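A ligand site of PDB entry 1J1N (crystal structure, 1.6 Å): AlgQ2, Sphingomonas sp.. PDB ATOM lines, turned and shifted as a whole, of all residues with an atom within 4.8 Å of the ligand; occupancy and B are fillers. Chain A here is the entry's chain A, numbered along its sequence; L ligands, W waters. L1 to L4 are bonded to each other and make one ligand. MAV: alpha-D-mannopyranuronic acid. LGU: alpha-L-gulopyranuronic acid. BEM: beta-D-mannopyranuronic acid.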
ATOM      1  N   ARG A  20     -29.470  -4.468  26.582  1.00  0.00           N
ATOM      2  CA  ARG A  20     -28.269  -4.650  27.387  1.00  0.00           C
ATOM      3  C   ARG A  20     -28.556  -5.213  28.773  1.00  0.00           C
ATOM      4  O   ARG A  20     -27.822  -4.941  29.729  1.00  0.00           O
ATOM      5  CB  ARG A  20     -27.509  -3.313  27.454  1.00  0.00           C
ATOM      6  CG  ARG A  20     -27.045  -2.858  26.068  1.00  0.00           C
ATOM      7  CD  ARG A  20     -26.509  -1.418  26.027  1.00  0.00           C
ATOM      8  NE  ARG A  20     -26.038  -1.109  24.677  1.00  0.00           N
ATOM      9  CZ  ARG A  20     -25.830   0.112  24.192  1.00  0.00           C
ATOM     10  NH1 ARG A  20     -26.045   1.174  24.956  1.00  0.00           N
ATOM     11  NH2 ARG A  20     -25.396   0.268  22.953  1.00  0.00           N
ATOM     12  N   ASP A  21     -29.618  -6.015  28.871  1.00  0.00           N
ATOM     13  CA  ASP A  21     -30.018  -6.674  30.114  1.00  0.00           C
ATOM     14  C   ASP A  21     -30.271  -5.727  31.287  1.00  0.00           C
ATOM     15  O   ASP A  21     -30.228  -6.167  32.436  1.00  0.00           O
ATOM     16  CB  ASP A  21     -28.960  -7.697  30.539  1.00  0.00           C
ATOM     17  CG  ASP A  21     -28.891  -8.900  29.615  1.00  0.00           C
ATOM     18  OD1 ASP A  21     -27.925  -9.681  29.734  1.00  0.00           O
ATOM     19  OD2 ASP A  21     -29.804  -9.069  28.777  1.00  0.00           O
ATOM     20  N   GLN A  55     -32.802 -10.648  25.640  1.00  0.00           N
ATOM     21  CA  GLN A  55     -33.163 -11.587  24.589  1.00  0.00           C
ATOM     22  C   GLN A  55     -34.376 -12.413  25.000  1.00  0.00           C
ATOM     23  O   GLN A  55     -35.243 -12.696  24.166  1.00  0.00           O
ATOM     24  CB  GLN A  55     -31.972 -12.491  24.243  1.00  0.00           C
ATOM     25  CG  GLN A  55     -30.808 -11.743  23.584  1.00  0.00           C
ATOM     26  CD  GLN A  55     -31.238 -10.989  22.338  1.00  0.00           C
ATOM     27  OE1 GLN A  55     -31.858 -11.561  21.434  1.00  0.00           O
ATOM     28  NE2 GLN A  55     -30.890  -9.708  22.262  1.00  0.00           N
ATOM     29  N   ASP A  74     -30.521  -4.202  21.349  1.00  0.00           N
ATOM     30  CA  ASP A  74     -29.211  -4.649  20.907  1.00  0.00           C
ATOM     31  C   ASP A  74     -29.224  -6.131  20.532  1.00  0.00           C
ATOM     32  O   ASP A  74     -30.017  -6.921  21.056  1.00  0.00           O
ATOM     33  CB  ASP A  74     -28.198  -4.450  22.023  1.00  0.00           C
ATOM     34  CG  ASP A  74     -28.534  -5.260  23.254  1.00  0.00           C
ATOM     35  OD1 ASP A  74     -29.575  -4.964  23.890  1.00  0.00           O
ATOM     36  OD2 ASP A  74     -27.779  -6.186  23.594  1.00  0.00           O
ATOM     37  N   ASN A  75     -28.324  -6.490  19.627  1.00  0.00           N
ATOM     38  CA  ASN A  75     -28.157  -7.873  19.197  1.00  0.00           C
ATOM     39  C   ASN A  75     -29.442  -8.553  18.750  1.00  0.00           C
ATOM     40  O   ASN A  75     -29.743  -9.676  19.140  1.00  0.00           O
ATOM     41  CB  ASN A  75     -27.516  -8.668  20.328  1.00  0.00           C
ATOM     42  CG  ASN A  75     -26.114  -8.170  20.649  1.00  0.00           C
ATOM     43  OD1 ASN A  75     -25.189  -8.343  19.864  1.00  0.00           O
ATOM     44  ND2 ASN A  75     -25.966  -7.523  21.805  1.00  0.00           N
ATOM     45  N   TYR A 129     -28.212   0.698  14.318  1.00  0.00           N
ATOM     46  CA  TYR A 129     -27.427   1.617  15.121  1.00  0.00           C
ATOM     47  C   TYR A 129     -26.105   1.622  14.347  1.00  0.00           C
ATOM     48  O   TYR A 129     -25.457   0.581  14.200  1.00  0.00           O
ATOM     49  CB  TYR A 129     -27.241   1.047  16.533  1.00  0.00           C
ATOM     50  CG  TYR A 129     -26.003   1.486  17.305  1.00  0.00           C
ATOM     51  CD1 TYR A 129     -25.387   2.712  17.062  1.00  0.00           C
ATOM     52  CD2 TYR A 129     -25.480   0.682  18.318  1.00  0.00           C
ATOM     53  CE1 TYR A 129     -24.282   3.129  17.799  1.00  0.00           C
ATOM     54  CE2 TYR A 129     -24.374   1.092  19.074  1.00  0.00           C
ATOM     55  CZ  TYR A 129     -23.780   2.308  18.806  1.00  0.00           C
ATOM     56  OH  TYR A 129     -22.694   2.709  19.559  1.00  0.00           O
ATOM     57  N   ARG A 137     -11.734  -1.221  21.636  1.00  0.00           N
ATOM     58  CA  ARG A 137     -10.981  -1.525  22.848  1.00  0.00           C
ATOM     59  C   ARG A 137      -9.467  -1.480  22.678  1.00  0.00           C
ATOM     60  O   ARG A 137      -8.941  -1.520  21.558  1.00  0.00           O
ATOM     61  CB  ARG A 137     -11.371  -2.899  23.386  1.00  0.00           C
ATOM     62  CG  ARG A 137     -12.806  -2.992  23.868  1.00  0.00           C
ATOM     63  CD  ARG A 137     -13.144  -4.415  24.307  1.00  0.00           C
ATOM     64  NE  ARG A 137     -14.495  -4.507  24.851  1.00  0.00           N
ATOM     65  CZ  ARG A 137     -15.606  -4.467  24.111  1.00  0.00           C
ATOM     66  NH1 ARG A 137     -15.529  -4.346  22.800  1.00  0.00           N
ATOM     67  NH2 ARG A 137     -16.792  -4.537  24.709  1.00  0.00           N
ATOM     68  N   ARG A 186     -15.252  -5.800  32.484  1.00  0.00           N
ATOM     69  CA  ARG A 186     -16.706  -5.742  32.607  1.00  0.00           C
ATOM     70  C   ARG A 186     -17.405  -6.651  31.587  1.00  0.00           C
ATOM     71  O   ARG A 186     -18.589  -6.945  31.732  1.00  0.00           O
ATOM     72  CB  ARG A 186     -17.209  -4.301  32.481  1.00  0.00           C
ATOM     73  CG  ARG A 186     -16.799  -3.594  31.225  1.00  0.00           C
ATOM     74  CD  ARG A 186     -17.636  -2.353  31.000  1.00  0.00           C
ATOM     75  NE  ARG A 186     -17.056  -1.515  29.953  1.00  0.00           N
ATOM     76  CZ  ARG A 186     -17.754  -0.697  29.162  1.00  0.00           C
ATOM     77  NH1 ARG A 186     -19.076  -0.597  29.295  1.00  0.00           N
ATOM     78  NH2 ARG A 186     -17.129   0.027  28.250  1.00  0.00           N
ATOM     79  N   HIS A 187     -16.675  -7.081  30.563  1.00  0.00           N
ATOM     80  CA  HIS A 187     -17.232  -8.005  29.583  1.00  0.00           C
ATOM     81  C   HIS A 187     -16.549  -9.342  29.798  1.00  0.00           C
ATOM     82  O   HIS A 187     -15.370  -9.498  29.507  1.00  0.00           O
ATOM     83  CB  HIS A 187     -17.011  -7.516  28.148  1.00  0.00           C
ATOM     84  CG  HIS A 187     -17.871  -6.356  27.759  1.00  0.00           C
ATOM     85  ND1 HIS A 187     -17.477  -5.047  27.921  1.00  0.00           N
ATOM     86  CD2 HIS A 187     -19.135  -6.317  27.277  1.00  0.00           C
ATOM     87  CE1 HIS A 187     -18.467  -4.241  27.563  1.00  0.00           C
ATOM     88  NE2 HIS A 187     -19.481  -4.988  27.160  1.00  0.00           N
ATOM     89  N   ASP A 189     -16.552 -12.005  28.197  1.00  0.00           N
ATOM     90  CA  ASP A 189     -16.010 -12.525  26.949  1.00  0.00           C
ATOM     91  C   ASP A 189     -14.551 -12.144  26.685  1.00  0.00           C
ATOM     92  O   ASP A 189     -13.862 -12.807  25.913  1.00  0.00           O
ATOM     93  CB  ASP A 189     -16.864 -12.050  25.782  1.00  0.00           C
ATOM     94  CG  ASP A 189     -18.339 -12.270  26.028  1.00  0.00           C
ATOM     95  OD1 ASP A 189     -18.910 -11.585  26.912  1.00  0.00           O
ATOM     96  OD2 ASP A 189     -18.934 -13.133  25.348  1.00  0.00           O
ATOM     97  N   TYR A 208     -18.520 -10.571  19.920  1.00  0.00           N
ATOM     98  CA  TYR A 208     -17.807 -11.710  20.488  1.00  0.00           C
ATOM     99  C   TYR A 208     -18.156 -13.032  19.807  1.00  0.00           C
ATOM    100  O   TYR A 208     -19.295 -13.236  19.369  1.00  0.00           O
ATOM    101  CB  TYR A 208     -18.060 -11.807  22.003  1.00  0.00           C
ATOM    102  CG  TYR A 208     -17.450 -10.677  22.795  1.00  0.00           C
ATOM    103  CD1 TYR A 208     -18.248  -9.737  23.440  1.00  0.00           C
ATOM    104  CD2 TYR A 208     -16.055 -10.540  22.888  1.00  0.00           C
ATOM    105  CE1 TYR A 208     -17.684  -8.687  24.169  1.00  0.00           C
ATOM    106  CE2 TYR A 208     -15.491  -9.489  23.617  1.00  0.00           C
ATOM    107  CZ  TYR A 208     -16.312  -8.563  24.246  1.00  0.00           C
ATOM    108  OH  TYR A 208     -15.760  -7.519  24.940  1.00  0.00           O
ATOM    109  N   TRP A 270     -12.723  -0.055  26.255  1.00  0.00           N
ATOM    110  CA  TRP A 270     -12.751   1.131  25.398  1.00  0.00           C
ATOM    111  C   TRP A 270     -11.878   2.282  25.892  1.00  0.00           C
ATOM    112  O   TRP A 270     -11.830   2.572  27.087  1.00  0.00           O
ATOM    113  CB  TRP A 270     -14.202   1.598  25.216  1.00  0.00           C
ATOM    114  CG  TRP A 270     -15.092   0.591  24.534  1.00  0.00           C
ATOM    115  CD1 TRP A 270     -15.538  -0.595  25.045  1.00  0.00           C
ATOM    116  CD2 TRP A 270     -15.638   0.689  23.213  1.00  0.00           C
ATOM    117  NE1 TRP A 270     -16.332  -1.235  24.122  1.00  0.00           N
ATOM    118  CE2 TRP A 270     -16.413  -0.475  22.991  1.00  0.00           C
ATOM    119  CE3 TRP A 270     -15.555   1.645  22.188  1.00  0.00           C
ATOM    120  CZ2 TRP A 270     -17.102  -0.702  21.791  1.00  0.00           C
ATOM    121  CZ3 TRP A 270     -16.234   1.417  20.987  1.00  0.00           C
ATOM    122  CH2 TRP A 270     -16.996   0.247  20.805  1.00  0.00           C
ATOM    123  N   PHE A 271     -11.207   2.959  24.957  1.00  0.00           N
ATOM    124  CA  PHE A 271     -10.326   4.078  25.296  1.00  0.00           C
ATOM    125  C   PHE A 271     -10.949   5.240  26.058  1.00  0.00           C
ATOM    126  O   PHE A 271     -10.445   5.641  27.103  1.00  0.00           O
ATOM    127  CB  PHE A 271      -9.671   4.615  24.021  1.00  0.00           C
ATOM    128  CG  PHE A 271      -8.550   3.755  23.501  1.00  0.00           C
ATOM    129  CD1 PHE A 271      -7.243   3.991  23.891  1.00  0.00           C
ATOM    130  CD2 PHE A 271      -8.814   2.708  22.617  1.00  0.00           C
ATOM    131  CE1 PHE A 271      -6.197   3.191  23.422  1.00  0.00           C
ATOM    132  CE2 PHE A 271      -7.778   1.899  22.145  1.00  0.00           C
ATOM    133  CZ  PHE A 271      -6.470   2.149  22.551  1.00  0.00           C
ATOM    134  N   ALA A 272     -12.049   5.774  25.538  1.00  0.00           N
ATOM    135  CA  ALA A 272     -12.692   6.929  26.167  1.00  0.00           C
ATOM    136  C   ALA A 272     -13.145   6.692  27.602  1.00  0.00           C
ATOM    137  O   ALA A 272     -12.691   7.374  28.528  1.00  0.00           O
ATOM    138  CB  ALA A 272     -13.855   7.420  25.317  1.00  0.00           C
ATOM    139  N   SER A 273     -14.045   5.736  27.811  1.00  0.00           N
ATOM    140  CA  SER A 273     -14.535   5.495  29.158  1.00  0.00           C
ATOM    141  C   SER A 273     -13.505   4.935  30.139  1.00  0.00           C
ATOM    142  O   SER A 273     -13.506   5.304  31.306  1.00  0.00           O
ATOM    143  CB  SER A 273     -15.770   4.581  29.132  1.00  0.00           C
ATOM    144  OG  SER A 273     -15.441   3.290  28.668  1.00  0.00           O
ATOM    145  N   ARG A 309     -13.979  -0.779  15.715  1.00  0.00           N
ATOM    146  CA  ARG A 309     -15.294  -0.152  15.679  1.00  0.00           C
ATOM    147  C   ARG A 309     -16.045  -0.710  14.473  1.00  0.00           C
ATOM    148  O   ARG A 309     -15.538  -0.705  13.351  1.00  0.00           O
ATOM    149  CB  ARG A 309     -15.143   1.368  15.552  1.00  0.00           C
ATOM    150  CG  ARG A 309     -16.418   2.166  15.749  1.00  0.00           C
ATOM    151  CD  ARG A 309     -16.671   2.491  17.214  1.00  0.00           C
ATOM    152  NE  ARG A 309     -15.544   3.183  17.838  1.00  0.00           N
ATOM    153  CZ  ARG A 309     -15.655   4.202  18.686  1.00  0.00           C
ATOM    154  NH1 ARG A 309     -16.851   4.670  19.012  1.00  0.00           N
ATOM    155  NH2 ARG A 309     -14.578   4.733  19.234  1.00  0.00           N
ATOM    156  N   ARG A 313     -23.700  -1.982  13.819  1.00  0.00           N
ATOM    157  CA  ARG A 313     -23.876  -2.998  14.845  1.00  0.00           C
ATOM    158  C   ARG A 313     -25.170  -3.767  14.611  1.00  0.00           C
ATOM    159  O   ARG A 313     -26.064  -3.305  13.897  1.00  0.00           O
ATOM    160  CB  ARG A 313     -23.882  -2.371  16.251  1.00  0.00           C
ATOM    161  CG  ARG A 313     -22.493  -2.359  16.932  1.00  0.00           C
ATOM    162  CD  ARG A 313     -22.605  -2.116  18.442  1.00  0.00           C
ATOM    163  NE  ARG A 313     -23.509  -3.086  19.048  1.00  0.00           N
ATOM    164  CZ  ARG A 313     -23.136  -4.228  19.622  1.00  0.00           C
ATOM    165  NH1 ARG A 313     -21.860  -4.574  19.692  1.00  0.00           N
ATOM    166  NH2 ARG A 313     -24.067  -5.065  20.068  1.00  0.00           N
ATOM    167  N   ASP A 315     -27.758  -4.044  16.087  1.00  0.00           N
ATOM    168  CA  ASP A 315     -28.753  -3.407  16.940  1.00  0.00           C
ATOM    169  C   ASP A 315     -29.629  -2.469  16.122  1.00  0.00           C
ATOM    170  O   ASP A 315     -29.246  -2.037  15.034  1.00  0.00           O
ATOM    171  CB  ASP A 315     -28.091  -2.533  18.024  1.00  0.00           C
ATOM    172  CG  ASP A 315     -26.913  -3.201  18.723  1.00  0.00           C
ATOM    173  OD1 ASP A 315     -26.757  -4.433  18.662  1.00  0.00           O
ATOM    174  OD2 ASP A 315     -26.153  -2.447  19.381  1.00  0.00           O
ATOM    175  N   ASN A 375     -20.952   8.469  28.166  1.00  0.00           N
ATOM    176  CA  ASN A 375     -21.922   7.552  27.591  1.00  0.00           C
ATOM    177  C   ASN A 375     -22.842   6.982  28.671  1.00  0.00           C
ATOM    178  O   ASN A 375     -24.054   6.854  28.452  1.00  0.00           O
ATOM    179  CB  ASN A 375     -21.274   6.440  26.729  1.00  0.00           C
ATOM    180  CG  ASN A 375     -20.159   5.667  27.431  1.00  0.00           C
ATOM    181  OD1 ASN A 375     -19.734   5.980  28.540  1.00  0.00           O
ATOM    182  ND2 ASN A 375     -19.667   4.630  26.750  1.00  0.00           N
ATOM    183  N   TYR A 379     -26.974   7.185  28.703  1.00  0.00           N
ATOM    184  CA  TYR A 379     -27.846   6.007  28.687  1.00  0.00           C
ATOM    185  C   TYR A 379     -29.051   6.245  29.590  1.00  0.00           C
ATOM    186  O   TYR A 379     -30.189   5.960  29.214  1.00  0.00           O
ATOM    187  CB  TYR A 379     -27.119   4.766  29.212  1.00  0.00           C
ATOM    188  CG  TYR A 379     -25.880   4.349  28.448  1.00  0.00           C
ATOM    189  CD1 TYR A 379     -25.775   4.527  27.073  1.00  0.00           C
ATOM    190  CD2 TYR A 379     -24.835   3.695  29.106  1.00  0.00           C
ATOM    191  CE1 TYR A 379     -24.664   4.063  26.362  1.00  0.00           C
ATOM    192  CE2 TYR A 379     -23.732   3.233  28.418  1.00  0.00           C
ATOM    193  CZ  TYR A 379     -23.647   3.412  27.044  1.00  0.00           C
ATOM    194  OH  TYR A 379     -22.566   2.918  26.355  1.00  0.00           O
ATOM    195  N   GLN A 384     -27.479   7.680  23.288  1.00  0.00           N
ATOM    196  CA  GLN A 384     -26.476   6.649  23.039  1.00  0.00           C
ATOM    197  C   GLN A 384     -27.075   5.271  23.305  1.00  0.00           C
ATOM    198  O   GLN A 384     -26.400   4.365  23.789  1.00  0.00           O
ATOM    199  CB  GLN A 384     -25.218   6.851  23.906  1.00  0.00           C
ATOM    200  CG  GLN A 384     -24.389   8.087  23.557  1.00  0.00           C
ATOM    201  CD  GLN A 384     -23.964   8.143  22.091  1.00  0.00           C
ATOM    202  OE1 GLN A 384     -23.676   7.121  21.482  1.00  0.00           O
ATOM    203  NE2 GLN A 384     -23.910   9.356  21.546  1.00  0.00           N
ATOM    204  N   GLN A 391     -24.658   7.393  14.879  1.00  0.00           N
ATOM    205  CA  GLN A 391     -23.780   7.943  15.902  1.00  0.00           C
ATOM    206  C   GLN A 391     -22.891   9.036  15.316  1.00  0.00           C
ATOM    207  O   GLN A 391     -22.550   9.001  14.131  1.00  0.00           O
ATOM    208  CB  GLN A 391     -22.923   6.840  16.521  1.00  0.00           C
ATOM    209  CG  GLN A 391     -22.260   7.263  17.827  1.00  0.00           C
ATOM    210  CD  GLN A 391     -21.500   6.130  18.504  1.00  0.00           C
ATOM    211  OE1 GLN A 391     -21.575   5.958  19.729  1.00  0.00           O
ATOM    212  NE2 GLN A 391     -20.755   5.361  17.717  1.00  0.00           N
ATOM    213  N   TYR A 395     -19.294  13.510  19.567  1.00  0.00           N
ATOM    214  CA  TYR A 395     -19.838  13.432  20.921  1.00  0.00           C
ATOM    215  C   TYR A 395     -18.758  12.806  21.795  1.00  0.00           C
ATOM    216  O   TYR A 395     -18.528  13.243  22.923  1.00  0.00           O
ATOM    217  CB  TYR A 395     -21.119  12.568  20.939  1.00  0.00           C
ATOM    218  CG  TYR A 395     -20.996  11.217  21.634  1.00  0.00           C
ATOM    219  CD1 TYR A 395     -21.219  11.100  23.009  1.00  0.00           C
ATOM    220  CD2 TYR A 395     -20.639  10.070  20.925  1.00  0.00           C
ATOM    221  CE1 TYR A 395     -21.096   9.866  23.656  1.00  0.00           C
ATOM    222  CE2 TYR A 395     -20.507   8.827  21.567  1.00  0.00           C
ATOM    223  CZ  TYR A 395     -20.730   8.736  22.931  1.00  0.00           C
ATOM    224  OH  TYR A 395     -20.596   7.524  23.576  1.00  0.00           O
ATOM    225  N   GLU A 396     -18.095  11.787  21.254  1.00  0.00           N
ATOM    226  CA  GLU A 396     -17.048  11.066  21.970  1.00  0.00           C
ATOM    227  C   GLU A 396     -15.754  11.859  22.041  1.00  0.00           C
ATOM    228  O   GLU A 396     -15.064  11.855  23.067  1.00  0.00           O
ATOM    229  CB  GLU A 396     -16.797   9.721  21.281  1.00  0.00           C
ATOM    230  CG  GLU A 396     -15.992   8.722  22.099  1.00  0.00           C
ATOM    231  CD  GLU A 396     -15.872   7.393  21.391  1.00  0.00           C
ATOM    232  OE1 GLU A 396     -16.888   6.918  20.832  1.00  0.00           O
ATOM    233  OE2 GLU A 396     -14.758   6.815  21.393  1.00  0.00           O
ATOM    234  N   TRP A 399     -15.185  14.090  25.136  1.00  0.00           N
ATOM    235  CA  TRP A 399     -14.814  13.576  26.442  1.00  0.00           C
ATOM    236  C   TRP A 399     -13.658  12.583  26.365  1.00  0.00           C
ATOM    237  O   TRP A 399     -13.411  11.813  27.287  1.00  0.00           O
ATOM    238  CB  TRP A 399     -16.016  12.983  27.201  1.00  0.00           C
ATOM    239  CG  TRP A 399     -16.818  11.945  26.502  1.00  0.00           C
ATOM    240  CD1 TRP A 399     -17.758  12.145  25.538  1.00  0.00           C
ATOM    241  CD2 TRP A 399     -16.806  10.532  26.763  1.00  0.00           C
ATOM    242  NE1 TRP A 399     -18.342  10.953  25.175  1.00  0.00           N
ATOM    243  CE2 TRP A 399     -17.774   9.947  25.916  1.00  0.00           C
ATOM    244  CE3 TRP A 399     -16.074   9.713  27.629  1.00  0.00           C
ATOM    245  CZ2 TRP A 399     -18.021   8.567  25.901  1.00  0.00           C
ATOM    246  CZ3 TRP A 399     -16.329   8.352  27.622  1.00  0.00           C
ATOM    247  CH2 TRP A 399     -17.297   7.793  26.764  1.00  0.00           C
HETATM  248  C1  MAV L   1     -26.587 -10.309  25.748  1.00  0.00           C
HETATM  249  O1  MAV L   1     -27.315 -10.002  24.601  1.00  0.00           O
HETATM  250  C2  MAV L   1     -26.604  -9.140  26.720  1.00  0.00           C
HETATM  251  O2  MAV L   1     -25.866  -9.473  27.877  1.00  0.00           O
HETATM  252  C3  MAV L   1     -25.997  -7.910  26.055  1.00  0.00           C
HETATM  253  O3  MAV L   1     -25.899  -6.845  26.999  1.00  0.00           O
HETATM  254  C4  MAV L   1     -24.600  -8.220  25.503  1.00  0.00           C
HETATM  255  O4  MAV L   1     -24.176  -7.102  24.691  1.00  0.00           O
HETATM  256  C5  MAV L   1     -24.619  -9.493  24.630  1.00  0.00           C
HETATM  257  O5  MAV L   1     -25.229 -10.589  25.341  1.00  0.00           O
HETATM  258  C6  MAV L   1     -23.216  -9.901  24.210  1.00  0.00           C
HETATM  259  O6A MAV L   1     -22.579 -10.666  24.962  1.00  0.00           O
HETATM  260  O6B MAV L   1     -22.773  -9.474  23.127  1.00  0.00           O
HETATM  261  C1  LGU L   2     -22.836  -6.732  24.755  1.00  0.00           C
HETATM  262  C2  LGU L   2     -22.473  -5.921  23.491  1.00  0.00           C
HETATM  263  O2  LGU L   2     -22.814  -6.669  22.346  1.00  0.00           O
HETATM  264  C3  LGU L   2     -23.213  -4.584  23.464  1.00  0.00           C
HETATM  265  O3  LGU L   2     -24.609  -4.793  23.232  1.00  0.00           O
HETATM  266  C4  LGU L   2     -23.031  -3.845  24.787  1.00  0.00           C
HETATM  267  O4  LGU L   2     -21.654  -3.435  24.931  1.00  0.00           O
HETATM  268  C5  LGU L   2     -23.401  -4.724  25.979  1.00  0.00           C
HETATM  269  O5  LGU L   2     -22.631  -5.950  25.943  1.00  0.00           O
HETATM  270  C6  LGU L   2     -23.121  -3.977  27.268  1.00  0.00           C
HETATM  271  O6B LGU L   2     -22.330  -4.478  28.091  1.00  0.00           O
HETATM  272  O6A LGU L   2     -23.665  -2.865  27.440  1.00  0.00           O
HETATM  273  C1  MAV L   3     -21.478  -2.064  24.794  1.00  0.00           C
HETATM  274  C2  MAV L   3     -20.158  -1.635  25.448  1.00  0.00           C
HETATM  275  O2  MAV L   3     -19.080  -2.293  24.788  1.00  0.00           O
HETATM  276  C3  MAV L   3     -20.016  -0.105  25.326  1.00  0.00           C
HETATM  277  O3  MAV L   3     -18.728   0.290  25.804  1.00  0.00           O
HETATM  278  C4  MAV L   3     -20.199   0.345  23.862  1.00  0.00           C
HETATM  279  O4  MAV L   3     -20.316   1.771  23.818  1.00  0.00           O
HETATM  280  C5  MAV L   3     -21.479  -0.227  23.287  1.00  0.00           C
HETATM  281  O5  MAV L   3     -21.495  -1.647  23.439  1.00  0.00           O
HETATM  282  C6  MAV L   3     -21.633   0.164  21.830  1.00  0.00           C
HETATM  283  O6A MAV L   3     -21.020  -0.490  20.968  1.00  0.00           O
HETATM  284  O6B MAV L   3     -22.340   1.158  21.580  1.00  0.00           O
HETATM  285  C1  BEM L   4     -19.227   2.501  23.395  1.00  0.00           C
HETATM  286  C2  BEM L   4     -19.757   3.802  22.776  1.00  0.00           C
HETATM  287  O2  BEM L   4     -20.608   4.430  23.706  1.00  0.00           O
HETATM  288  C3  BEM L   4     -18.583   4.701  22.507  1.00  0.00           C
HETATM  289  O3  BEM L   4     -18.957   5.915  21.865  1.00  0.00           O
HETATM  290  C4  BEM L   4     -17.566   4.798  23.581  1.00  0.00           C
HETATM  291  C5  BEM L   4     -17.347   3.655  24.413  1.00  0.00           C
HETATM  292  O5  BEM L   4     -18.448   2.760  24.582  1.00  0.00           O
HETATM  293  C6  BEM L   4     -16.551   3.819  25.592  1.00  0.00           C
HETATM  294  O6B BEM L   4     -16.888   3.151  26.588  1.00  0.00           O
HETATM  295  O6A BEM L   4     -15.575   4.597  25.564  1.00  0.00           O
HETATM  296  O   HOH W   1     -18.984  -4.514  22.792  1.00  0.00           O
HETATM  297  O   HOH W   2     -20.679  -9.399  26.537  1.00  0.00           O
HETATM  298  O   HOH W   3     -21.194 -12.797  24.066  1.00  0.00           O
HETATM  299  O   HOH W   4     -27.232 -11.876  22.687  1.00  0.00           O
HETATM  300  O   HOH W   5     -13.969   4.858  23.362  1.00  0.00           O
HETATM  301  O   HOH W   6     -24.716  -6.775  29.824  1.00  0.00           O
HETATM  302  O   HOH W   7     -20.204   0.639  18.673  1.00  0.00           O
HETATM  303  O   HOH W   8     -25.595  -2.390  22.016  1.00  0.00           O
HETATM  304  O   HOH W   9     -29.578  -8.313  24.422  1.00  0.00           O
HETATM  305  O   HOH W  10     -22.480  -7.968  19.564  1.00  0.00           O
HETATM  306  O   HOH W  11     -23.907  -0.667  28.760  1.00  0.00           O
HETATM  307  O   HOH W  12     -21.024  -9.441  21.213  1.00  0.00           O
HETATM  308  O   HOH W  13     -22.986   2.973  23.640  1.00  0.00           O
HETATM  309  O   HOH W  14     -24.190 -13.511  24.597  1.00  0.00           O
HETATM  310  O   HOH W  15     -19.788  -2.875  20.755  1.00  0.00           O
HETATM  311  O   HOH W  16     -19.890  -6.659  21.381  1.00  0.00           O
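O3 of BEM L4 is in hydrogen-bond range of OE1 of Glu 396 (2.5 Å). An oxygen (O6A) of BEM L4 sits at hydrogen-bond distance from the backbone NH (N) of Ser 273 (2.9 Å). The side-chain hydroxyl of Ser 273 is in hydrogen-bond range of an oxygen (O6B) of BEM L4, at 2.5 Å. An oxygen (O6B) of MAV L3 sits at hydrogen-bond distance from the side-chain hydroxyl of Tyr 129. OD1 of Asp 21 lies within hydrogen-bond range of O2 of MAV L1 (2.8 Å). An oxygen (O3) of BEM L4 lies within hydrogen-bond range of the side-chain hydroxyl (OH) of Tyr 395 (2.9 Å). The guanidinium group of Arg 186 is in salt-bridge range of an oxygen (O6B) of BEM L4 (3.5 Å). The indole nitrogen (NE1) of Trp 270 lies within hydrogen-bond range of an oxygen (O2) of MAV L3 (3.0 Å). O6B of LGU L2 lies within hydrogen-bond range of NE2 of His 187, at 3.0 Å. NH2 of Arg 313 is in hydrogen-bond range of O2 of LGU L2, 3.1 Å away. ND2 of Asn 375 sits at hydrogen-bond distance from O5 of BEM L4, 3.1 Å away. The guanidinium group (NH2) of Arg 137 lies within hydrogen-bond range of an oxygen (O2) of MAV L3 (3.2 Å). The guanidinium group (NH2) of Arg 20 is in salt-bridge range of an oxygen (O6B) of MAV L3 (3.5 Å). An oxygen (O2) of LGU L2 sits at hydrogen-bond distance from the side-chain amide nitrogen (ND2) of Asn 75, at 3.3 Å. An oxygen (O3) of BEM L4 is in hydrogen-bond range of the side-chain amide oxygen (OE1) of Gln 391, at 3.4 Å. The side-chain carboxylate (OD2) of Asp 74 is in hydrogen-bond range of an oxygen (O3) of LGU L2, at 3.5 Å.
Residues that only touch the ligand: Ala 272 (3.3 Å), Arg 309 (3.8 Å), Tyr 379 (3.6 Å) and Trp 399 (3.8 Å). The nearest printed residue that does not touch the ligand is Gln 55 (4.03 Å).
The backbone carbonyl oxygen of Tyr 129 is in hydrogen-bond range of the backbone NH of Arg 313 (3.1 Å). OH of Tyr 129 sits at hydrogen-bond distance from OE1 of Gln 391 (3.4 Å). The guanidinium group (NE) of Arg 313 is in salt-bridge range of the side-chain carboxylate (OD2) of Asp 315 (2.7 Å). The side-chain hydroxyl (OH) of Tyr 379 sits at hydrogen-bond distance from the side-chain amide nitrogen (ND2) of Asn 375 (3.4 Å). OH of Tyr 208 is in hydrogen-bond range of NH2 of Arg 137, at 3.2 Å. The backbone NH (N) of Arg 20 sits at hydrogen-bond distance from the side-chain carboxylate (OD1) of Asp 74, at 2.7 Å. The guanidinium group (NH1) of Arg 20 is in hydrogen-bond range of the backbone carbonyl oxygen (O) of Gln 384 (3.4 Å). The side-chain amide oxygen (OE1) of Gln 391 sits close to the side-chain amide oxygen (OE1) of Gln 384.
Water W12 lies within hydrogen-bond range of an oxygen (O6B) of MAV L1 (2.6 Å) and the backbone NH of Tyr 208 (3.0 Å). Water W7 lies within hydrogen-bond range of an oxygen (O6A) of MAV L3 (2.7 Å) and the side-chain hydroxyl (OH) of Tyr 129 (3.4 Å). Water W5 lies within hydrogen-bond range of an oxygen (O6A) of BEM L4, the side-chain carboxylate (OE2) of Glu 396 and the backbone NH (N) of Ala 272. Water W13 lies within hydrogen-bond range of the side-chain hydroxyl of Tyr 379 and an oxygen (O2) of BEM L4. Water W16 lies within hydrogen-bond range of an oxygen (O2) of LGU L2 and the guanidinium group of Arg 313. Water W10 lies within hydrogen-bond range of the side-chain amide oxygen of Asn 75 (2.8 Å), an oxygen (O2) of LGU L2 (3.1 Å) and the guanidinium group of Arg 313 (3.3 Å).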
